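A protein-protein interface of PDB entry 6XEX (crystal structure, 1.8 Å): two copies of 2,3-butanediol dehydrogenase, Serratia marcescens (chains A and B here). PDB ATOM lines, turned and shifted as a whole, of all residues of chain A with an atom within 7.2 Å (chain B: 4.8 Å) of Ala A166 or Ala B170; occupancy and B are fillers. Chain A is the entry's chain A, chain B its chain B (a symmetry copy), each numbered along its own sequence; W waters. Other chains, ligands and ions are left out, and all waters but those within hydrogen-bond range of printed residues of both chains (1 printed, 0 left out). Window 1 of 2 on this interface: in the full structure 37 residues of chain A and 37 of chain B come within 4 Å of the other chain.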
ATOM      1  N   TRP A 117       0.372  -9.835  -1.551  1.00  0.00           N
ATOM      2  CA  TRP A 117       0.716  -9.415  -0.178  1.00  0.00           C
ATOM      3  C   TRP A 117       0.806  -7.899  -0.142  1.00  0.00           C
ATOM      4  O   TRP A 117       0.256  -7.291   0.771  1.00  0.00           O
ATOM      5  CB  TRP A 117       2.027 -10.050   0.303  1.00  0.00           C
ATOM      6  CG  TRP A 117       2.550  -9.434   1.553  1.00  0.00           C
ATOM      7  CD1 TRP A 117       3.760  -8.840   1.715  1.00  0.00           C
ATOM      8  CD2 TRP A 117       1.908  -9.361   2.834  1.00  0.00           C
ATOM      9  NE1 TRP A 117       3.918  -8.427   3.002  1.00  0.00           N
ATOM     10  CE2 TRP A 117       2.791  -8.707   3.707  1.00  0.00           C
ATOM     11  CE3 TRP A 117       0.660  -9.767   3.321  1.00  0.00           C
ATOM     12  CZ2 TRP A 117       2.489  -8.455   5.036  1.00  0.00           C
ATOM     13  CZ3 TRP A 117       0.334  -9.477   4.623  1.00  0.00           C
ATOM     14  CH2 TRP A 117       1.254  -8.872   5.480  1.00  0.00           C
ATOM     15  N   ILE A 120      -2.688  -6.300  -0.332  1.00  0.00           N
ATOM     16  CA  ILE A 120      -3.400  -6.540   0.966  1.00  0.00           C
ATOM     17  C   ILE A 120      -2.807  -5.654   2.068  1.00  0.00           C
ATOM     18  O   ILE A 120      -3.550  -4.946   2.772  1.00  0.00           O
ATOM     19  CB  ILE A 120      -3.332  -8.040   1.326  1.00  0.00           C
ATOM     20  CG1 ILE A 120      -4.195  -8.897   0.401  1.00  0.00           C
ATOM     21  CG2 ILE A 120      -3.683  -8.252   2.802  1.00  0.00           C
ATOM     22  CD1 ILE A 120      -5.685  -8.790   0.653  1.00  0.00           C
ATOM     23  N   ILE A 125      -3.656  -2.759   6.010  1.00  0.00           N
ATOM     24  CA  ILE A 125      -2.847  -2.412   7.205  1.00  0.00           C
ATOM     25  C   ILE A 125      -2.464  -0.936   7.084  1.00  0.00           C
ATOM     26  O   ILE A 125      -2.810  -0.150   7.956  1.00  0.00           O
ATOM     27  CB  ILE A 125      -1.600  -3.320   7.415  1.00  0.00           C
ATOM     28  CG1 ILE A 125      -1.905  -4.811   7.213  1.00  0.00           C
ATOM     29  CG2 ILE A 125      -1.013  -3.067   8.784  1.00  0.00           C
ATOM     30  CD1 ILE A 125      -0.704  -5.709   7.269  1.00  0.00           C
ATOM     31  N   SER A 153     -11.719 -12.634  10.532  1.00  0.00           N
ATOM     32  CA  SER A 153     -10.389 -13.082  10.063  1.00  0.00           C
ATOM     33  C   SER A 153      -9.227 -12.289  10.701  1.00  0.00           C
ATOM     34  O   SER A 153      -8.071 -12.590  10.367  1.00  0.00           O
ATOM     35  CB  SER A 153     -10.335 -12.991   8.539  1.00  0.00           C
ATOM     36  OG  SER A 153     -11.433 -13.625   7.931  1.00  0.00           O
ATOM     37  N   GLY A 154      -9.476 -11.315  11.580  1.00  0.00           N
ATOM     38  CA  GLY A 154      -8.430 -10.689  12.412  1.00  0.00           C
ATOM     39  C   GLY A 154      -8.417 -11.254  13.810  1.00  0.00           C
ATOM     40  O   GLY A 154      -7.405 -11.130  14.488  1.00  0.00           O
ATOM     41  N   GLY A 156      -9.098 -14.593  14.390  1.00  0.00           N
ATOM     42  CA  GLY A 156      -8.616 -15.956  14.216  1.00  0.00           C
ATOM     43  C   GLY A 156      -8.199 -16.146  12.773  1.00  0.00           C
ATOM     44  O   GLY A 156      -8.412 -15.207  11.965  1.00  0.00           O
ATOM     45  N   ALA A 161      -6.796 -17.722   3.388  1.00  0.00           N
ATOM     46  CA  ALA A 161      -6.718 -16.245   3.270  1.00  0.00           C
ATOM     47  C   ALA A 161      -5.562 -15.717   4.117  1.00  0.00           C
ATOM     48  O   ALA A 161      -5.791 -14.861   4.994  1.00  0.00           O
ATOM     49  CB  ALA A 161      -8.052 -15.626   3.625  1.00  0.00           C
ATOM     50  N   ALA A 162      -4.366 -16.242   3.894  1.00  0.00           N
ATOM     51  CA  ALA A 162      -3.246 -16.071   4.868  1.00  0.00           C
ATOM     52  C   ALA A 162      -2.879 -14.583   4.996  1.00  0.00           C
ATOM     53  O   ALA A 162      -2.754 -14.047   6.122  1.00  0.00           O
ATOM     54  CB  ALA A 162      -2.079 -16.915   4.456  1.00  0.00           C
ATOM     55  N   TYR A 163      -2.713 -13.901   3.870  1.00  0.00           N
ATOM     56  CA  TYR A 163      -2.272 -12.492   3.861  1.00  0.00           C
ATOM     57  C   TYR A 163      -3.364 -11.644   4.504  1.00  0.00           C
ATOM     58  O   TYR A 163      -3.069 -10.769   5.336  1.00  0.00           O
ATOM     59  CB  TYR A 163      -1.988 -11.978   2.450  1.00  0.00           C
ATOM     60  CG  TYR A 163      -0.845 -12.644   1.720  1.00  0.00           C
ATOM     61  CD1 TYR A 163       0.204 -13.286   2.369  1.00  0.00           C
ATOM     62  CD2 TYR A 163      -0.824 -12.651   0.326  1.00  0.00           C
ATOM     63  CE1 TYR A 163       1.235 -13.906   1.676  1.00  0.00           C
ATOM     64  CE2 TYR A 163       0.210 -13.251  -0.373  1.00  0.00           C
ATOM     65  CZ  TYR A 163       1.236 -13.894   0.293  1.00  0.00           C
ATOM     66  OH  TYR A 163       2.231 -14.524  -0.398  1.00  0.00           O
ATOM     67  N   TYR A 164      -4.620 -11.884   4.114  1.00  0.00           N
ATOM     68  CA  TYR A 164      -5.807 -11.176   4.682  1.00  0.00           C
ATOM     69  C   TYR A 164      -5.824 -11.333   6.217  1.00  0.00           C
ATOM     70  O   TYR A 164      -6.115 -10.378   6.926  1.00  0.00           O
ATOM     71  CB  TYR A 164      -7.095 -11.711   4.054  1.00  0.00           C
ATOM     72  CG  TYR A 164      -8.352 -10.991   4.471  1.00  0.00           C
ATOM     73  CD1 TYR A 164      -8.601  -9.709   3.998  1.00  0.00           C
ATOM     74  CD2 TYR A 164      -9.331 -11.606   5.247  1.00  0.00           C
ATOM     75  CE1 TYR A 164      -9.762  -9.031   4.340  1.00  0.00           C
ATOM     76  CE2 TYR A 164     -10.515 -10.942   5.587  1.00  0.00           C
ATOM     77  CZ  TYR A 164     -10.708  -9.647   5.140  1.00  0.00           C
ATOM     78  OH  TYR A 164     -11.846  -8.957   5.400  1.00  0.00           O
ATOM     79  N   CYS A 165      -5.589 -12.534   6.723  1.00  0.00           N
ATOM     80  CA  CYS A 165      -5.588 -12.814   8.188  1.00  0.00           C
ATOM     81  C   CYS A 165      -4.446 -12.037   8.869  1.00  0.00           C
ATOM     82  O   CYS A 165      -4.657 -11.542   9.987  1.00  0.00           O
ATOM     83  CB  CYS A 165      -5.516 -14.302   8.454  1.00  0.00           C
ATOM     84  SG  CYS A 165      -7.064 -15.140   8.025  1.00  0.00           S
ATOM     85  N   ALA A 166      -3.281 -11.967   8.249  1.00  0.00           N
ATOM     86  CA  ALA A 166      -2.156 -11.177   8.796  1.00  0.00           C
ATOM     87  C   ALA A 166      -2.593  -9.716   8.928  1.00  0.00           C
ATOM     88  O   ALA A 166      -2.343  -9.072   9.977  1.00  0.00           O
ATOM     89  CB  ALA A 166      -0.936 -11.369   7.934  1.00  0.00           C
ATOM     90  N   ALA A 167      -3.159  -9.160   7.854  1.00  0.00           N
ATOM     91  CA  ALA A 167      -3.597  -7.757   7.804  1.00  0.00           C
ATOM     92  C   ALA A 167      -4.665  -7.506   8.866  1.00  0.00           C
ATOM     93  O   ALA A 167      -4.555  -6.512   9.635  1.00  0.00           O
ATOM     94  CB  ALA A 167      -4.069  -7.404   6.405  1.00  0.00           C
ATOM     95  N   LYS A 168      -5.729  -8.323   8.894  1.00  0.00           N
ATOM     96  CA  LYS A 168      -6.827  -8.047   9.833  1.00  0.00           C
ATOM     97  C   LYS A 168      -6.328  -8.300  11.262  1.00  0.00           C
ATOM     98  O   LYS A 168      -6.786  -7.572  12.218  1.00  0.00           O
ATOM     99  CB  LYS A 168      -8.060  -8.861   9.445  1.00  0.00           C
ATOM    100  CG  LYS A 168      -8.698  -8.428   8.146  1.00  0.00           C
ATOM    101  CD  LYS A 168      -9.165  -6.963   8.192  1.00  0.00           C
ATOM    102  CE  LYS A 168     -10.037  -6.609   7.005  1.00  0.00           C
ATOM    103  NZ  LYS A 168     -10.428  -5.191   7.065  1.00  0.00           N
ATOM    104  N   GLY A 169      -5.391  -9.229  11.435  1.00  0.00           N
ATOM    105  CA  GLY A 169      -4.759  -9.441  12.746  1.00  0.00           C
ATOM    106  C   GLY A 169      -4.057  -8.177  13.222  1.00  0.00           C
ATOM    107  O   GLY A 169      -4.057  -7.853  14.413  1.00  0.00           O
ATOM    108  N   ALA A 170      -3.395  -7.491  12.304  1.00  0.00           N
ATOM    109  CA  ALA A 170      -2.694  -6.234  12.624  1.00  0.00           C
ATOM    110  C   ALA A 170      -3.729  -5.188  13.049  1.00  0.00           C
ATOM    111  O   ALA A 170      -3.551  -4.469  14.061  1.00  0.00           O
ATOM    112  CB  ALA A 170      -1.942  -5.822  11.397  1.00  0.00           C
ATOM    113  N   VAL A 171      -4.836  -5.117  12.325  1.00  0.00           N
ATOM    114  CA  VAL A 171      -5.909  -4.120  12.625  1.00  0.00           C
ATOM    115  C   VAL A 171      -6.461  -4.331  14.031  1.00  0.00           C
ATOM    116  O   VAL A 171      -6.558  -3.369  14.846  1.00  0.00           O
ATOM    117  CB  VAL A 171      -6.992  -4.159  11.541  1.00  0.00           C
ATOM    118  CG1 VAL A 171      -8.130  -3.224  11.944  1.00  0.00           C
ATOM    119  CG2 VAL A 171      -6.415  -3.798  10.195  1.00  0.00           C
ATOM    120  N   VAL A 172      -6.797  -5.578  14.381  1.00  0.00           N
ATOM    121  CA  VAL A 172      -7.310  -5.928  15.731  1.00  0.00           C
ATOM    122  C   VAL A 172      -6.369  -5.447  16.831  1.00  0.00           C
ATOM    123  O   VAL A 172      -6.837  -4.902  17.804  1.00  0.00           O
ATOM    124  CB  VAL A 172      -7.515  -7.455  15.758  1.00  0.00           C
ATOM    125  CG1 VAL A 172      -7.543  -8.084  17.129  1.00  0.00           C
ATOM    126  CG2 VAL A 172      -8.771  -7.765  14.966  1.00  0.00           C
ATOM    127  N   ASN A 173      -5.082  -5.707  16.731  1.00  0.00           N
ATOM    128  CA  ASN A 173      -4.168  -5.357  17.824  1.00  0.00           C
ATOM    129  C   ASN A 173      -3.750  -3.870  17.740  1.00  0.00           C
ATOM    130  O   ASN A 173      -3.510  -3.308  18.815  1.00  0.00           O
ATOM    131  CB  ASN A 173      -2.947  -6.270  17.886  1.00  0.00           C
ATOM    132  CG  ASN A 173      -2.499  -6.415  19.325  1.00  0.00           C
ATOM    133  OD1 ASN A 173      -3.356  -6.624  20.185  1.00  0.00           O
ATOM    134  ND2 ASN A 173      -1.190  -6.395  19.608  1.00  0.00           N
ATOM    135  N   ILE B 125       6.803  -8.213  10.188  1.00  0.00           N
ATOM    136  CA  ILE B 125       5.701  -8.843   9.426  1.00  0.00           C
ATOM    137  C   ILE B 125       6.265  -9.475   8.166  1.00  0.00           C
ATOM    138  O   ILE B 125       6.038 -10.689   7.955  1.00  0.00           O
ATOM    139  CB  ILE B 125       4.566  -7.881   9.090  1.00  0.00           C
ATOM    140  CG1 ILE B 125       4.173  -6.997  10.270  1.00  0.00           C
ATOM    141  CG2 ILE B 125       3.388  -8.695   8.555  1.00  0.00           C
ATOM    142  CD1 ILE B 125       3.202  -5.927   9.878  1.00  0.00           C
ATOM    143  N   ALA B 166       0.831  -3.677  16.245  1.00  0.00           N
ATOM    144  CA  ALA B 166       0.183  -4.011  14.972  1.00  0.00           C
ATOM    145  C   ALA B 166       0.963  -5.151  14.304  1.00  0.00           C
ATOM    146  O   ALA B 166       0.350  -6.100  13.809  1.00  0.00           O
ATOM    147  CB  ALA B 166       0.020  -2.780  14.113  1.00  0.00           C
ATOM    148  N   ALA B 167       2.290  -5.075  14.283  1.00  0.00           N
ATOM    149  CA  ALA B 167       3.153  -6.031  13.571  1.00  0.00           C
ATOM    150  C   ALA B 167       3.070  -7.376  14.300  1.00  0.00           C
ATOM    151  O   ALA B 167       2.885  -8.410  13.650  1.00  0.00           O
ATOM    152  CB  ALA B 167       4.577  -5.516  13.489  1.00  0.00           C
ATOM    153  N   LYS B 168       3.211  -7.389  15.611  1.00  0.00           N
ATOM    154  CA  LYS B 168       3.169  -8.660  16.357  1.00  0.00           C
ATOM    155  C   LYS B 168       1.749  -9.249  16.324  1.00  0.00           C
ATOM    156  O   LYS B 168       1.674 -10.490  16.343  1.00  0.00           O
ATOM    157  CB  LYS B 168       3.731  -8.479  17.766  1.00  0.00           C
ATOM    158  CG  LYS B 168       5.240  -8.264  17.809  1.00  0.00           C
ATOM    159  CD  LYS B 168       6.089  -9.382  17.246  1.00  0.00           C
ATOM    160  CE  LYS B 168       7.581  -9.160  17.430  1.00  0.00           C
ATOM    161  NZ  LYS B 168       8.347 -10.302  16.904  1.00  0.00           N
ATOM    162  N   GLY B 169       0.698  -8.421  16.330  1.00  0.00           N
ATOM    163  CA  GLY B 169      -0.696  -8.864  16.081  1.00  0.00           C
ATOM    164  C   GLY B 169      -0.813  -9.623  14.757  1.00  0.00           C
ATOM    165  O   GLY B 169      -1.528 -10.643  14.711  1.00  0.00           O
ATOM    166  N   ALA B 170      -0.194  -9.093  13.683  1.00  0.00           N
ATOM    167  CA  ALA B 170      -0.139  -9.741  12.365  1.00  0.00           C
ATOM    168  C   ALA B 170       0.535 -11.108  12.494  1.00  0.00           C
ATOM    169  O   ALA B 170       0.036 -12.093  11.963  1.00  0.00           O
ATOM    170  CB  ALA B 170       0.547  -8.849  11.345  1.00  0.00           C
ATOM    171  N   VAL B 171       1.617 -11.197  13.249  1.00  0.00           N
ATOM    172  CA  VAL B 171       2.357 -12.483  13.370  1.00  0.00           C
ATOM    173  C   VAL B 171       1.476 -13.502  14.102  1.00  0.00           C
ATOM    174  O   VAL B 171       1.421 -14.649  13.694  1.00  0.00           O
ATOM    175  CB  VAL B 171       3.721 -12.281  14.050  1.00  0.00           C
ATOM    176  CG1 VAL B 171       4.450 -13.601  14.253  1.00  0.00           C
ATOM    177  CG2 VAL B 171       4.574 -11.329  13.230  1.00  0.00           C
ATOM    178  N   VAL B 172       0.836 -13.103  15.190  1.00  0.00           N
ATOM    179  CA  VAL B 172      -0.029 -14.033  15.973  1.00  0.00           C
ATOM    180  C   VAL B 172      -1.128 -14.598  15.058  1.00  0.00           C
ATOM    181  O   VAL B 172      -1.347 -15.795  15.128  1.00  0.00           O
ATOM    182  CB  VAL B 172      -0.584 -13.272  17.178  1.00  0.00           C
ATOM    183  CG1 VAL B 172      -1.858 -13.837  17.763  1.00  0.00           C
ATOM    184  CG2 VAL B 172       0.521 -13.126  18.229  1.00  0.00           C
ATOM    185  N   ASN B 173      -1.811 -13.759  14.268  1.00  0.00           N
ATOM    186  CA  ASN B 173      -2.945 -14.245  13.430  1.00  0.00           C
ATOM    187  C   ASN B 173      -2.435 -14.928  12.169  1.00  0.00           C
ATOM    188  O   ASN B 173      -3.098 -15.892  11.719  1.00  0.00           O
ATOM    189  CB  ASN B 173      -3.954 -13.155  13.119  1.00  0.00           C
ATOM    190  CG  ASN B 173      -5.353 -13.714  13.008  1.00  0.00           C
ATOM    191  OD1 ASN B 173      -5.754 -14.514  13.861  1.00  0.00           O
ATOM    192  ND2 ASN B 173      -6.021 -13.421  11.893  1.00  0.00           N
ATOM    193  N   LEU B 174      -1.294 -14.501  11.618  1.00  0.00           N
ATOM    194  CA  LEU B 174      -0.674 -15.236  10.483  1.00  0.00           C
ATOM    195  C   LEU B 174      -0.276 -16.644  10.928  1.00  0.00           C
ATOM    196  O   LEU B 174      -0.486 -17.591  10.155  1.00  0.00           O
ATOM    197  CB  LEU B 174       0.570 -14.501   9.951  1.00  0.00           C
ATOM    198  CG  LEU B 174       1.302 -15.134   8.765  1.00  0.00           C
ATOM    199  CD1 LEU B 174       0.434 -15.241   7.523  1.00  0.00           C
ATOM    200  CD2 LEU B 174       2.557 -14.317   8.432  1.00  0.00           C
ATOM    201  N   THR B 175       0.219 -16.811  12.157  1.00  0.00           N
ATOM    202  CA  THR B 175       0.570 -18.131  12.714  1.00  0.00           C
ATOM    203  C   THR B 175      -0.681 -18.996  12.624  1.00  0.00           C
ATOM    204  O   THR B 175      -0.575 -20.155  12.183  1.00  0.00           O
ATOM    205  CB  THR B 175       1.066 -18.007  14.155  1.00  0.00           C
ATOM    206  OG1 THR B 175       2.260 -17.221  14.107  1.00  0.00           O
ATOM    207  CG2 THR B 175       1.295 -19.342  14.825  1.00  0.00           C
HETATM  208  O   HOH W   1      -3.918 -10.095  16.159  1.00  0.00           O
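Water W1 bridges O of Gly A169 and O of Gly B169.
Trp A117 touches Ile B125. O of Gly A154 touches CG of Asn B173, 3.6 Å away. Ala A162 touches Leu B174 (O to CD1, 3.7 Å). Ala A166 touches Ala B170. O of Gly A169 touches C of Gly B169, at 3.7 Å. C of Gly A169 touches N of Ala B170, 3.997 Å away. Gly A169 touches Asn B173 (CA to CB, 3.8 Å). CA of Ala A170 touches O of Ala B166 (3.3 Å). Ala B170 touches Ala A170. CB of Asn A173 touches CA of Gly B169 (3.9 Å).
The side-chain sulfur (SG) of Cys A165 sits close to the backbone carbonyl oxygen (O) of Ser A153 (3.6 Å). O of Ala A161 is in hydrogen-bond range of SG of Cys A165, 3.3 Å away.
Ala A166 touches Ala B170, and with the chains exchanged Ala A170 touches Ala B166. Gly B169 touches its own counterpart, Gly A169. Gly A169 touches Ala B170, but with the chains exchanged Ala A170 does not touch Gly B169 (4.2 Å). Gly A169 touches Asn B173, and with the chains exchanged Asn A173 touches Gly B169.
Hydrophobic or aromatic side chains of chain B within 4 Å of the printed part of chain A: Ile B125, Ala B166, Ala B170 and Leu B174. Among the printed residues, no Asp or Glu carboxylate lies within 4 Å of a Lys or Arg side-chain nitrogen of the other chain.
Of the printed residues of chain B, Ala A166 touches Ala B170 (3.2 Å). Of chain A, only Gly A169 and Asn A173 come within 4 Å of Gly B169. Printed residues of chain B within 4 Å of Gly A169: Gly B169, Ala B170 and Asn B173. Of the printed residues of chain A, Ile B125 touches Trp A117 (3.6 Å). Of the printed residues of chain B, Gly A154 touches Asn B173. Val B172 touches none of the printed residues of chain A. Val A172 touches none of the printed residues of chain B. The nearest printed residue of chain B that does not touch Ala A166 is Leu B174 (4.02 Å). The nearest printed residue of chain A that does not touch Asn B173 is Ala A166 (4.8 Å).
The side-chain amide nitrogen of Asn B173 sits at hydrogen-bond distance from the backbone carbonyl oxygen of Ser A153, at 2.7 Å. ND2 of Asn B173 is in hydrogen-bond range of O of Gly A156 (3.0 Å). The side-chain amide nitrogen (ND2) of Asn B173 lies within hydrogen-bond range of the backbone carbonyl oxygen (O) of Cys A165 (3.0 Å).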
